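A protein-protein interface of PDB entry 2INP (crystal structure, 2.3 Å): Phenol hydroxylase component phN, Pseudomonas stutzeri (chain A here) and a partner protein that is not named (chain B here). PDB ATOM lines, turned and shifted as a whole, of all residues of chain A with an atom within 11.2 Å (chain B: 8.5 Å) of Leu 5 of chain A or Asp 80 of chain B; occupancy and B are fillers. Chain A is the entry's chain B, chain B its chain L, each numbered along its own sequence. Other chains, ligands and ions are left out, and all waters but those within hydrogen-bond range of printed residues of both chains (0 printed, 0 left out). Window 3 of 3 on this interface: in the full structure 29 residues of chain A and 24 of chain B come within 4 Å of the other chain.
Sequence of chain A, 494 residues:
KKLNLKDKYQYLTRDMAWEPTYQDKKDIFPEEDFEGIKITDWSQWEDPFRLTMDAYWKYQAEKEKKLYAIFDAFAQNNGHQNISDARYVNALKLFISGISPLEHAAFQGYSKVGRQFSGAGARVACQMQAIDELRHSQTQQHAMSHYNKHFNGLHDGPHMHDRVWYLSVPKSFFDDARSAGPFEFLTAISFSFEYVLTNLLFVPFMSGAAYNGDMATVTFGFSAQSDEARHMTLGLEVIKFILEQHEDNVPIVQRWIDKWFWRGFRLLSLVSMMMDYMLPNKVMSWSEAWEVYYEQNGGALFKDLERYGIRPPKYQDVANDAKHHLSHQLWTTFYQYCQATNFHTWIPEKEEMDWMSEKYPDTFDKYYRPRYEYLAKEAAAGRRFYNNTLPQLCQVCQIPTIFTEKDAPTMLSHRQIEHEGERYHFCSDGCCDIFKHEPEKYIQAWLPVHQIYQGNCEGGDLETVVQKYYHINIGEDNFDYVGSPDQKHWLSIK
Leu 5 of chain A touches Asp 80 of chain B.
Val 77 of chain B touches Pro 48 of chain A (CG1 to O, 3.7 Å).
Arg 50 of chain A touches Gln 64 of chain B.
Leu 51 of chain A touches Gln 64 of chain B (CD2 to NE2, 3.4 Å).
Gln 64 of chain B touches Tyr 59 of chain A (CB to CE2, 3.8 Å).
OH of Tyr 9 of chain A lies within hydrogen-bond range of O of Leu 51 of chain A (3.0 Å).
The side-chain carboxylate (OD1) of Asp 47 of chain A lies within salt-bridge range of the guanidinium group (NH2) of Arg 50 of chain A (2.9 Å).
The side-chain carboxylate (OD2) of Asp 62 of chain B is in hydrogen-bond range of the backbone NH (N) of Gln 64 of chain B, 3.3 Å away.
Printed residues of chain B within 4 Å of Leu 5 of chain A: Asp 80 (3.6 Å).
No residue of chain A comes within 4 Å of Asp 78 of chain B.
No residue of chain A comes within 4 Å of Glu 79 of chain B.
No residue of chain A comes within 4 Å of His 83 of chain B.
Of the printed residues of chain A, Asp 62 of chain B touches Tyr 59.
Of the printed residues of chain A, Gln 64 of chain B touches Arg 50, Leu 51 and Tyr 59.
Of the printed residues of chain B, Arg 50 of chain A touches Gln 64 (3.8 Å).
Printed residues of chain B within 4 Å of Leu 51 of chain A: Gln 64.
The nearest residue of chain A that does not touch Asp 80 of chain B is Arg 50 of chain A (6.9 Å).
The nearest printed residue of chain B that does not touch Arg 50 of chain A is Glu 79 of chain B (4.9 Å).
Hydrophobic or aromatic side chains of chain B that line the printed part of chain A: Val 77.
Of the 22 printed residues of chain A, 5 touch a printed residue of chain B.
Printed residues of chain A that touch a printed residue of chain B: Leu 5, Pro 48, Arg 50, Leu 51 and Tyr 59.
Among the printed residues, 6 pairs touch across the chains.
The side-chain hydroxyl (OH) of Tyr 59 of chain A is in hydrogen-bond range of the side-chain carboxylate (OD1) of Asp 62 of chain B, at 2.8 Å.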
ATOM      1  N   LYS A   1      -5.531  11.193  20.457  1.00  0.00           N
ATOM      2  CA  LYS A   1      -6.160  12.282  19.630  1.00  0.00           C
ATOM      3  C   LYS A   1      -6.570  11.808  18.224  1.00  0.00           C
ATOM      4  O   LYS A   1      -5.692  11.747  17.333  1.00  0.00           O
ATOM      5  CB  LYS A   1      -5.196  13.531  19.538  1.00  0.00           C
ATOM      6  N   LYS A   2      -7.877  11.526  18.035  1.00  0.00           N
ATOM      7  CA  LYS A   2      -8.433  10.903  16.793  1.00  0.00           C
ATOM      8  C   LYS A   2      -8.177  11.655  15.488  1.00  0.00           C
ATOM      9  O   LYS A   2      -8.148  12.885  15.474  1.00  0.00           O
ATOM     10  CB  LYS A   2      -9.931  10.663  16.903  1.00  0.00           C
ATOM     11  CG  LYS A   2     -10.292   9.482  17.723  1.00  0.00           C
ATOM     12  CD  LYS A   2     -11.326   8.701  16.990  1.00  0.00           C
ATOM     13  CE  LYS A   2     -11.745   7.477  17.815  1.00  0.00           C
ATOM     14  NZ  LYS A   2     -12.416   6.454  16.937  1.00  0.00           N
ATOM     15  N   LEU A   3      -7.997  10.922  14.389  1.00  0.00           N
ATOM     16  CA  LEU A   3      -7.605  11.548  13.116  1.00  0.00           C
ATOM     17  C   LEU A   3      -8.786  12.227  12.389  1.00  0.00           C
ATOM     18  O   LEU A   3      -9.855  11.625  12.279  1.00  0.00           O
ATOM     19  CB  LEU A   3      -6.935  10.521  12.189  1.00  0.00           C
ATOM     20  CG  LEU A   3      -5.506  10.110  12.500  1.00  0.00           C
ATOM     21  CD1 LEU A   3      -5.107   8.841  11.721  1.00  0.00           C
ATOM     22  CD2 LEU A   3      -4.517  11.283  12.284  1.00  0.00           C
ATOM     23  N   ASN A   4      -8.599  13.455  11.879  1.00  0.00           N
ATOM     24  CA  ASN A   4      -9.643  14.003  10.959  1.00  0.00           C
ATOM     25  C   ASN A   4      -9.592  13.395   9.551  1.00  0.00           C
ATOM     26  O   ASN A   4      -8.588  12.754   9.172  1.00  0.00           O
ATOM     27  CB  ASN A   4      -9.710  15.556  10.910  1.00  0.00           C
ATOM     28  CG  ASN A   4      -8.446  16.205  10.336  1.00  0.00           C
ATOM     29  OD1 ASN A   4      -8.037  17.257  10.807  1.00  0.00           O
ATOM     30  ND2 ASN A   4      -7.820  15.576   9.329  1.00  0.00           N
ATOM     31  N   LEU A   5     -10.680  13.553   8.806  1.00  0.00           N
ATOM     32  CA  LEU A   5     -10.765  13.078   7.384  1.00  0.00           C
ATOM     33  C   LEU A   5      -9.535  13.345   6.538  1.00  0.00           C
ATOM     34  O   LEU A   5      -9.053  12.424   5.897  1.00  0.00           O
ATOM     35  CB  LEU A   5     -11.984  13.654   6.658  1.00  0.00           C
ATOM     36  CG  LEU A   5     -13.266  13.098   7.249  1.00  0.00           C
ATOM     37  CD1 LEU A   5     -14.417  13.555   6.391  1.00  0.00           C
ATOM     38  CD2 LEU A   5     -13.193  11.531   7.381  1.00  0.00           C
ATOM     39  N   LYS A   6      -9.040  14.589   6.543  1.00  0.00           N
ATOM     40  CA  LYS A   6      -7.774  14.913   5.893  1.00  0.00           C
ATOM     41  C   LYS A   6      -6.572  14.083   6.335  1.00  0.00           C
ATOM     42  O   LYS A   6      -5.841  13.581   5.479  1.00  0.00           O
ATOM     43  CB  LYS A   6      -7.435  16.388   5.975  1.00  0.00           C
ATOM     44  CG  LYS A   6      -6.060  16.709   5.342  1.00  0.00           C
ATOM     45  CD  LYS A   6      -5.750  18.219   5.297  1.00  0.00           C
ATOM     46  CE  LYS A   6      -4.249  18.560   5.105  1.00  0.00           C
ATOM     47  NZ  LYS A   6      -4.199  20.015   4.716  1.00  0.00           N
ATOM     48  N   ASP A   7      -6.367  13.953   7.646  1.00  0.00           N
ATOM     49  CA  ASP A   7      -5.116  13.366   8.197  1.00  0.00           C
ATOM     50  C   ASP A   7      -5.091  11.840   8.077  1.00  0.00           C
ATOM     51  O   ASP A   7      -4.003  11.261   7.910  1.00  0.00           O
ATOM     52  CB  ASP A   7      -4.916  13.733   9.688  1.00  0.00           C
ATOM     53  CG  ASP A   7      -4.595  15.217   9.911  1.00  0.00           C
ATOM     54  OD1 ASP A   7      -3.918  15.840   9.048  1.00  0.00           O
ATOM     55  OD2 ASP A   7      -5.054  15.738  10.962  1.00  0.00           O
ATOM     56  N   LYS A   8      -6.283  11.235   8.171  1.00  0.00           N
ATOM     57  CA  LYS A   8      -6.520   9.809   8.030  1.00  0.00           C
ATOM     58  C   LYS A   8      -6.182   9.328   6.653  1.00  0.00           C
ATOM     59  O   LYS A   8      -5.615   8.260   6.476  1.00  0.00           O
ATOM     60  CB  LYS A   8      -7.972   9.460   8.252  1.00  0.00           C
ATOM     61  CG  LYS A   8      -8.144   7.976   8.373  1.00  0.00           C
ATOM     62  CD  LYS A   8      -9.526   7.607   8.853  1.00  0.00           C
ATOM     63  CE  LYS A   8      -9.922   6.255   8.245  1.00  0.00           C
ATOM     64  NZ  LYS A   8     -10.394   5.277   9.291  1.00  0.00           N
ATOM     65  N   TYR A   9      -6.543  10.137   5.679  1.00  0.00           N
ATOM     66  CA  TYR A   9      -6.338   9.815   4.308  1.00  0.00           C
ATOM     67  C   TYR A   9      -4.881   9.963   3.921  1.00  0.00           C
ATOM     68  O   TYR A   9      -4.347   9.168   3.133  1.00  0.00           O
ATOM     69  CB  TYR A   9      -7.203  10.730   3.441  1.00  0.00           C
ATOM     70  CG  TYR A   9      -7.061  10.363   1.971  1.00  0.00           C
ATOM     71  CD1 TYR A   9      -6.329  11.147   1.083  1.00  0.00           C
ATOM     72  CD2 TYR A   9      -7.586   9.168   1.529  1.00  0.00           C
ATOM     73  CE1 TYR A   9      -6.191  10.751  -0.200  1.00  0.00           C
ATOM     74  CE2 TYR A   9      -7.451   8.780   0.282  1.00  0.00           C
ATOM     75  CZ  TYR A   9      -6.785   9.554  -0.583  1.00  0.00           C
ATOM     76  OH  TYR A   9      -6.736   9.043  -1.839  1.00  0.00           O
ATOM     77  N   GLN A  10      -4.232  10.984   4.444  1.00  0.00           N
ATOM     78  CA  GLN A  10      -2.806  11.099   4.231  1.00  0.00           C
ATOM     79  C   GLN A  10      -2.029   9.939   4.899  1.00  0.00           C
ATOM     80  O   GLN A  10      -1.017   9.472   4.334  1.00  0.00           O
ATOM     81  CB  GLN A  10      -2.313  12.492   4.645  1.00  0.00           C
ATOM     82  CG  GLN A  10      -3.147  13.582   3.880  1.00  0.00           C
ATOM     83  CD  GLN A  10      -2.494  14.978   3.701  1.00  0.00           C
ATOM     84  OE1 GLN A  10      -3.031  15.819   2.949  1.00  0.00           O
ATOM     85  NE2 GLN A  10      -1.358  15.222   4.347  1.00  0.00           N
ATOM     86  N   TYR A  11      -2.542   9.458   6.051  1.00  0.00           N
ATOM     87  CA  TYR A  11      -2.059   8.268   6.696  1.00  0.00           C
ATOM     88  C   TYR A  11      -2.235   7.044   5.815  1.00  0.00           C
ATOM     89  O   TYR A  11      -1.343   6.233   5.774  1.00  0.00           O
ATOM     90  CB  TYR A  11      -2.651   8.038   8.084  1.00  0.00           C
ATOM     91  CG  TYR A  11      -1.729   8.575   9.183  1.00  0.00           C
ATOM     92  CD1 TYR A  11      -2.120   9.665   9.997  1.00  0.00           C
ATOM     93  CD2 TYR A  11      -0.466   8.012   9.400  1.00  0.00           C
ATOM     94  CE1 TYR A  11      -1.278  10.157  11.019  1.00  0.00           C
ATOM     95  CE2 TYR A  11       0.387   8.478  10.402  1.00  0.00           C
ATOM     96  CZ  TYR A  11      -0.026   9.551  11.232  1.00  0.00           C
ATOM     97  OH  TYR A  11       0.826  10.029  12.222  1.00  0.00           O
ATOM     98  N   LEU A  12      -3.326   6.978   5.060  1.00  0.00           N
ATOM     99  CA  LEU A  12      -3.589   5.853   4.176  1.00  0.00           C
ATOM    100  C   LEU A  12      -2.929   5.974   2.798  1.00  0.00           C
ATOM    101  O   LEU A  12      -2.993   5.047   1.998  1.00  0.00           O
ATOM    102  CB  LEU A  12      -5.080   5.619   4.022  1.00  0.00           C
ATOM    103  CG  LEU A  12      -5.777   5.215   5.329  1.00  0.00           C
ATOM    104  CD1 LEU A  12      -7.305   5.239   5.191  1.00  0.00           C
ATOM    105  CD2 LEU A  12      -5.268   3.839   5.841  1.00  0.00           C
ATOM    106  N   THR A  13      -2.283   7.102   2.521  1.00  0.00           N
ATOM    107  CA  THR A  13      -1.617   7.283   1.255  1.00  0.00           C
ATOM    108  C   THR A  13      -0.205   7.780   1.544  1.00  0.00           C
ATOM    109  O   THR A  13       0.702   6.956   1.679  1.00  0.00           O
ATOM    110  CB  THR A  13      -2.464   8.179   0.271  1.00  0.00           C
ATOM    111  OG1 THR A  13      -2.841   9.393   0.923  1.00  0.00           O
ATOM    112  CG2 THR A  13      -3.758   7.455  -0.137  1.00  0.00           C
ATOM    113  N   ARG A  14       0.010   9.089   1.673  1.00  0.00           N
ATOM    114  CA  ARG A  14       1.365   9.660   1.921  1.00  0.00           C
ATOM    115  C   ARG A  14       2.257   8.956   3.006  1.00  0.00           C
ATOM    116  O   ARG A  14       3.471   8.834   2.845  1.00  0.00           O
ATOM    117  CB  ARG A  14       1.227  11.144   2.325  1.00  0.00           C
ATOM    118  CG  ARG A  14       0.295  11.897   1.433  1.00  0.00           C
ATOM    119  CD  ARG A  14       0.405  13.371   1.652  1.00  0.00           C
ATOM    120  NE  ARG A  14      -0.505  14.077   0.754  1.00  0.00           N
ATOM    121  CZ  ARG A  14      -0.534  15.400   0.600  1.00  0.00           C
ATOM    122  NH1 ARG A  14      -1.416  15.935  -0.227  1.00  0.00           N
ATOM    123  NH2 ARG A  14       0.317  16.183   1.271  1.00  0.00           N
ATOM    124  N   GLU A  46      -2.604  19.485  -1.816  1.00  0.00           N
ATOM    125  CA  GLU A  46      -3.916  19.156  -1.264  1.00  0.00           C
ATOM    126  C   GLU A  46      -4.535  18.073  -2.104  1.00  0.00           C
ATOM    127  O   GLU A  46      -4.619  18.214  -3.304  1.00  0.00           O
ATOM    128  CB  GLU A  46      -4.871  20.369  -1.278  1.00  0.00           C
ATOM    129  CG  GLU A  46      -4.615  21.426  -0.155  1.00  0.00           C
ATOM    130  CD  GLU A  46      -4.843  20.883   1.272  1.00  0.00           C
ATOM    131  OE1 GLU A  46      -5.913  20.281   1.550  1.00  0.00           O
ATOM    132  OE2 GLU A  46      -3.938  21.084   2.121  1.00  0.00           O
ATOM    133  N   ASP A  47      -5.027  17.021  -1.473  1.00  0.00           N
ATOM    134  CA  ASP A  47      -5.746  15.971  -2.208  1.00  0.00           C
ATOM    135  C   ASP A  47      -6.985  16.489  -2.955  1.00  0.00           C
ATOM    136  O   ASP A  47      -8.004  16.841  -2.349  1.00  0.00           O
ATOM    137  CB  ASP A  47      -6.098  14.823  -1.280  1.00  0.00           C
ATOM    138  CG  ASP A  47      -4.875  14.284  -0.511  1.00  0.00           C
ATOM    139  OD1 ASP A  47      -4.886  14.359   0.743  1.00  0.00           O
ATOM    140  OD2 ASP A  47      -3.915  13.778  -1.151  1.00  0.00           O
ATOM    141  N   PRO A  48      -6.919  16.497  -4.305  1.00  0.00           N
ATOM    142  CA  PRO A  48      -8.095  16.981  -5.024  1.00  0.00           C
ATOM    143  C   PRO A  48      -9.402  16.288  -4.578  1.00  0.00           C
ATOM    144  O   PRO A  48     -10.433  16.960  -4.461  1.00  0.00           O
ATOM    145  CB  PRO A  48      -7.742  16.691  -6.506  1.00  0.00           C
ATOM    146  CG  PRO A  48      -6.656  15.679  -6.485  1.00  0.00           C
ATOM    147  CD  PRO A  48      -5.858  16.060  -5.238  1.00  0.00           C
ATOM    148  N   PHE A  49      -9.321  14.976  -4.304  1.00  0.00           N
ATOM    149  CA  PHE A  49     -10.396  14.078  -3.826  1.00  0.00           C
ATOM    150  C   PHE A  49      -9.694  13.102  -2.859  1.00  0.00           C
ATOM    151  O   PHE A  49      -8.420  12.999  -2.881  1.00  0.00           O
ATOM    152  CB  PHE A  49     -11.041  13.273  -5.011  1.00  0.00           C
ATOM    153  CG  PHE A  49     -10.003  12.715  -6.042  1.00  0.00           C
ATOM    154  CD1 PHE A  49      -9.443  11.408  -5.894  1.00  0.00           C
ATOM    155  CD2 PHE A  49      -9.597  13.486  -7.144  1.00  0.00           C
ATOM    156  CE1 PHE A  49      -8.493  10.898  -6.819  1.00  0.00           C
ATOM    157  CE2 PHE A  49      -8.632  12.983  -8.077  1.00  0.00           C
ATOM    158  CZ  PHE A  49      -8.094  11.680  -7.904  1.00  0.00           C
ATOM    159  N   ARG A  50     -10.497  12.393  -2.048  1.00  0.00           N
ATOM    160  CA  ARG A  50      -9.971  11.466  -1.075  1.00  0.00           C
ATOM    161  C   ARG A  50     -10.553  10.044  -1.244  1.00  0.00           C
ATOM    162  O   ARG A  50     -11.159   9.551  -0.317  1.00  0.00           O
ATOM    163  CB  ARG A  50     -10.278  11.942   0.358  1.00  0.00           C
ATOM    164  CG  ARG A  50      -9.647  13.258   0.775  1.00  0.00           C
ATOM    165  CD  ARG A  50      -9.843  13.673   2.236  1.00  0.00           C
ATOM    166  NE  ARG A  50      -9.704  15.156   2.263  1.00  0.00           N
ATOM    167  CZ  ARG A  50      -8.528  15.796   2.102  1.00  0.00           C
ATOM    168  NH1 ARG A  50      -8.464  17.121   2.095  1.00  0.00           N
ATOM    169  NH2 ARG A  50      -7.384  15.108   1.957  1.00  0.00           N
ATOM    170  N   LEU A  51     -10.341   9.347  -2.370  1.00  0.00           N
ATOM    171  CA  LEU A  51     -10.862   7.942  -2.488  1.00  0.00           C
ATOM    172  C   LEU A  51      -9.831   6.911  -2.051  1.00  0.00           C
ATOM    173  O   LEU A  51      -8.705   6.941  -2.515  1.00  0.00           O
ATOM    174  CB  LEU A  51     -11.329   7.604  -3.905  1.00  0.00           C
ATOM    175  CG  LEU A  51     -12.726   7.947  -4.322  1.00  0.00           C
ATOM    176  CD1 LEU A  51     -12.838   7.809  -5.846  1.00  0.00           C
ATOM    177  CD2 LEU A  51     -13.775   7.064  -3.600  1.00  0.00           C
ATOM    178  N   THR A  52     -10.194   6.014  -1.148  1.00  0.00           N
ATOM    179  CA  THR A  52      -9.331   4.889  -0.881  1.00  0.00           C
ATOM    180  C   THR A  52      -9.644   3.819  -1.941  1.00  0.00           C
ATOM    181  O   THR A  52     -10.624   3.933  -2.642  1.00  0.00           O
ATOM    182  CB  THR A  52      -9.461   4.361   0.566  1.00  0.00           C
ATOM    183  OG1 THR A  52     -10.817   4.244   0.911  1.00  0.00           O
ATOM    184  CG2 THR A  52      -8.813   5.286   1.535  1.00  0.00           C
ATOM    185  N   TYR A  59     -17.422   1.907  -5.833  1.00  0.00           N
ATOM    186  CA  TYR A  59     -18.271   2.885  -6.484  1.00  0.00           C
ATOM    187  C   TYR A  59     -18.135   2.779  -7.999  1.00  0.00           C
ATOM    188  O   TYR A  59     -19.103   2.897  -8.702  1.00  0.00           O
ATOM    189  CB  TYR A  59     -17.917   4.260  -5.926  1.00  0.00           C
ATOM    190  CG  TYR A  59     -18.437   4.387  -4.513  1.00  0.00           C
ATOM    191  CD1 TYR A  59     -19.816   4.368  -4.274  1.00  0.00           C
ATOM    192  CD2 TYR A  59     -17.567   4.479  -3.409  1.00  0.00           C
ATOM    193  CE1 TYR A  59     -20.299   4.464  -3.009  1.00  0.00           C
ATOM    194  CE2 TYR A  59     -18.033   4.583  -2.152  1.00  0.00           C
ATOM    195  CZ  TYR A  59     -19.406   4.603  -1.950  1.00  0.00           C
ATOM    196  OH  TYR A  59     -19.957   4.727  -0.660  1.00  0.00           O
ATOM    197  N   ILE B  48     -23.945  20.479  -1.499  1.00  0.00           N
ATOM    198  CA  ILE B  48     -24.778  19.400  -0.975  1.00  0.00           C
ATOM    199  C   ILE B  48     -24.401  19.167   0.500  1.00  0.00           C
ATOM    200  O   ILE B  48     -23.235  19.276   0.879  1.00  0.00           O
ATOM    201  CB  ILE B  48     -24.610  18.094  -1.817  1.00  0.00           C
ATOM    202  N   ARG B  50     -25.022  16.253   3.560  1.00  0.00           N
ATOM    203  CA  ARG B  50     -25.543  14.932   3.896  1.00  0.00           C
ATOM    204  C   ARG B  50     -26.940  15.046   4.526  1.00  0.00           C
ATOM    205  O   ARG B  50     -27.825  14.227   4.257  1.00  0.00           O
ATOM    206  CB  ARG B  50     -24.583  14.190   4.829  1.00  0.00           C
ATOM    207  N   TRP B  61     -27.155   8.469   4.141  1.00  0.00           N
ATOM    208  CA  TRP B  61     -26.635   8.686   2.809  1.00  0.00           C
ATOM    209  C   TRP B  61     -25.199   9.233   2.878  1.00  0.00           C
ATOM    210  O   TRP B  61     -24.927  10.213   3.584  1.00  0.00           O
ATOM    211  CB  TRP B  61     -27.574   9.617   2.034  1.00  0.00           C
ATOM    212  CG  TRP B  61     -27.157   9.940   0.608  1.00  0.00           C
ATOM    213  CD1 TRP B  61     -27.502   9.257  -0.534  1.00  0.00           C
ATOM    214  CD2 TRP B  61     -26.350  11.047   0.180  1.00  0.00           C
ATOM    215  NE1 TRP B  61     -26.947   9.865  -1.639  1.00  0.00           N
ATOM    216  CE2 TRP B  61     -26.236  10.964  -1.229  1.00  0.00           C
ATOM    217  CE3 TRP B  61     -25.704  12.095   0.852  1.00  0.00           C
ATOM    218  CZ2 TRP B  61     -25.503  11.890  -1.973  1.00  0.00           C
ATOM    219  CZ3 TRP B  61     -24.972  13.012   0.110  1.00  0.00           C
ATOM    220  CH2 TRP B  61     -24.886  12.908  -1.290  1.00  0.00           C
ATOM    221  N   ASP B  62     -24.291   8.571   2.155  1.00  0.00           N
ATOM    222  CA  ASP B  62     -22.886   8.972   2.086  1.00  0.00           C
ATOM    223  C   ASP B  62     -22.598   9.798   0.830  1.00  0.00           C
ATOM    224  O   ASP B  62     -23.186   9.561  -0.242  1.00  0.00           O
ATOM    225  CB  ASP B  62     -21.945   7.738   2.214  1.00  0.00           C
ATOM    226  CG  ASP B  62     -20.547   7.957   1.591  1.00  0.00           C
ATOM    227  OD1 ASP B  62     -20.179   7.163   0.690  1.00  0.00           O
ATOM    228  OD2 ASP B  62     -19.812   8.894   1.988  1.00  0.00           O
ATOM    229  N   VAL B  63     -21.689  10.766   0.991  1.00  0.00           N
ATOM    230  CA  VAL B  63     -21.238  11.665  -0.082  1.00  0.00           C
ATOM    231  C   VAL B  63     -20.729  10.891  -1.293  1.00  0.00           C
ATOM    232  O   VAL B  63     -21.265  11.047  -2.402  1.00  0.00           O
ATOM    233  CB  VAL B  63     -20.105  12.641   0.386  1.00  0.00           C
ATOM    234  CG1 VAL B  63     -20.110  13.930  -0.454  1.00  0.00           C
ATOM    235  CG2 VAL B  63     -20.217  12.967   1.874  1.00  0.00           C
ATOM    236  N   GLN B  64     -19.701  10.064  -1.074  1.00  0.00           N
ATOM    237  CA  GLN B  64     -19.020   9.327  -2.150  1.00  0.00           C
ATOM    238  C   GLN B  64     -20.009   8.649  -3.116  1.00  0.00           C
ATOM    239  O   GLN B  64     -19.639   8.265  -4.234  1.00  0.00           O
ATOM    240  CB  GLN B  64     -18.023   8.295  -1.571  1.00  0.00           C
ATOM    241  CG  GLN B  64     -16.717   8.884  -0.964  1.00  0.00           C
ATOM    242  CD  GLN B  64     -15.892   7.869  -0.156  1.00  0.00           C
ATOM    243  OE1 GLN B  64     -16.418   7.117   0.656  1.00  0.00           O
ATOM    244  NE2 GLN B  64     -14.594   7.873  -0.366  1.00  0.00           N
ATOM    245  N   VAL B  77     -12.977  21.892  -5.130  1.00  0.00           N
ATOM    246  CA  VAL B  77     -13.721  20.850  -4.422  1.00  0.00           C
ATOM    247  C   VAL B  77     -13.464  20.828  -2.923  1.00  0.00           C
ATOM    248  O   VAL B  77     -12.315  20.768  -2.475  1.00  0.00           O
ATOM    249  CB  VAL B  77     -13.574  19.447  -5.086  1.00  0.00           C
ATOM    250  CG1 VAL B  77     -13.836  18.293  -4.095  1.00  0.00           C
ATOM    251  CG2 VAL B  77     -14.524  19.343  -6.292  1.00  0.00           C
ATOM    252  N   ASP B  78     -14.555  20.890  -2.153  1.00  0.00           N
ATOM    253  CA  ASP B  78     -14.471  20.780  -0.708  1.00  0.00           C
ATOM    254  C   ASP B  78     -15.476  19.753  -0.166  1.00  0.00           C
ATOM    255  O   ASP B  78     -16.665  20.051  -0.004  1.00  0.00           O
ATOM    256  CB  ASP B  78     -14.661  22.156  -0.058  1.00  0.00           C
ATOM    257  CG  ASP B  78     -14.548  22.121   1.462  1.00  0.00           C
ATOM    258  OD1 ASP B  78     -14.356  21.032   2.055  1.00  0.00           O
ATOM    259  OD2 ASP B  78     -14.660  23.210   2.064  1.00  0.00           O
ATOM    260  N   GLU B  79     -14.969  18.553   0.125  1.00  0.00           N
ATOM    261  CA  GLU B  79     -15.769  17.452   0.645  1.00  0.00           C
ATOM    262  C   GLU B  79     -15.387  17.110   2.103  1.00  0.00           C
ATOM    263  O   GLU B  79     -14.191  17.158   2.488  1.00  0.00           O
ATOM    264  CB  GLU B  79     -15.634  16.227  -0.279  1.00  0.00           C
ATOM    265  CG  GLU B  79     -16.681  15.121  -0.077  1.00  0.00           C
ATOM    266  CD  GLU B  79     -16.371  13.837  -0.870  1.00  0.00           C
ATOM    267  OE1 GLU B  79     -15.431  13.855  -1.686  1.00  0.00           O
ATOM    268  OE2 GLU B  79     -17.067  12.805  -0.691  1.00  0.00           O
ATOM    269  N   ASP B  80     -16.414  16.779   2.897  1.00  0.00           N
ATOM    270  CA  ASP B  80     -16.255  16.426   4.315  1.00  0.00           C
ATOM    271  C   ASP B  80     -17.150  15.241   4.671  1.00  0.00           C
ATOM    272  O   ASP B  80     -17.674  14.559   3.789  1.00  0.00           O
ATOM    273  CB  ASP B  80     -16.573  17.618   5.227  1.00  0.00           C
ATOM    274  N   HIS B  83     -19.615  17.212   3.962  1.00  0.00           N
ATOM    275  CA  HIS B  83     -20.297  17.934   2.868  1.00  0.00           C
ATOM    276  C   HIS B  83     -19.701  17.696   1.465  1.00  0.00           C
ATOM    277  O   HIS B  83     -18.680  17.017   1.293  1.00  0.00           O
ATOM    278  CB  HIS B  83     -20.361  19.450   3.159  1.00  0.00           C
ATOM    279  CG  HIS B  83     -19.030  20.069   3.458  1.00  0.00           C
ATOM    280  ND1 HIS B  83     -18.640  20.412   4.733  1.00  0.00           N
ATOM    281  CD2 HIS B  83     -17.996  20.401   2.649  1.00  0.00           C
ATOM    282  CE1 HIS B  83     -17.421  20.924   4.701  1.00  0.00           C
ATOM    283  NE2 HIS B  83     -17.013  20.937   3.444  1.00  0.00           N
ATOM    284  N   PHE B  84     -20.371  18.246   0.460  1.00  0.00           N
ATOM    285  CA  PHE B  84     -19.749  18.402  -0.850  1.00  0.00           C
ATOM    286  C   PHE B  84     -20.055  19.799  -1.427  1.00  0.00           C
ATOM    287  O   PHE B  84     -21.200  20.138  -1.711  1.00  0.00           O
ATOM    288  CB  PHE B  84     -20.172  17.281  -1.807  1.00  0.00           C
ATOM    289  CG  PHE B  84     -19.262  17.132  -2.996  1.00  0.00           C
ATOM    290  CD1 PHE B  84     -18.393  16.057  -3.081  1.00  0.00           C
ATOM    291  CD2 PHE B  84     -19.252  18.087  -4.010  1.00  0.00           C
ATOM    292  CE1 PHE B  84     -17.552  15.917  -4.170  1.00  0.00           C
ATOM    293  CE2 PHE B  84     -18.415  17.969  -5.079  1.00  0.00           C
ATOM    294  CZ  PHE B  84     -17.554  16.875  -5.169  1.00  0.00           C
ATOM    295  N   ILE B  85     -19.025  20.616  -1.588  1.00  0.00           N
ATOM    296  CA  ILE B  85     -19.230  22.008  -1.996  1.00  0.00           C
ATOM    297  C   ILE B  85     -18.288  22.417  -3.142  1.00  0.00           C
ATOM    298  O   ILE B  85     -17.081  22.147  -3.103  1.00  0.00           O
ATOM    299  CB  ILE B  85     -19.076  22.945  -0.783  1.00  0.00           C
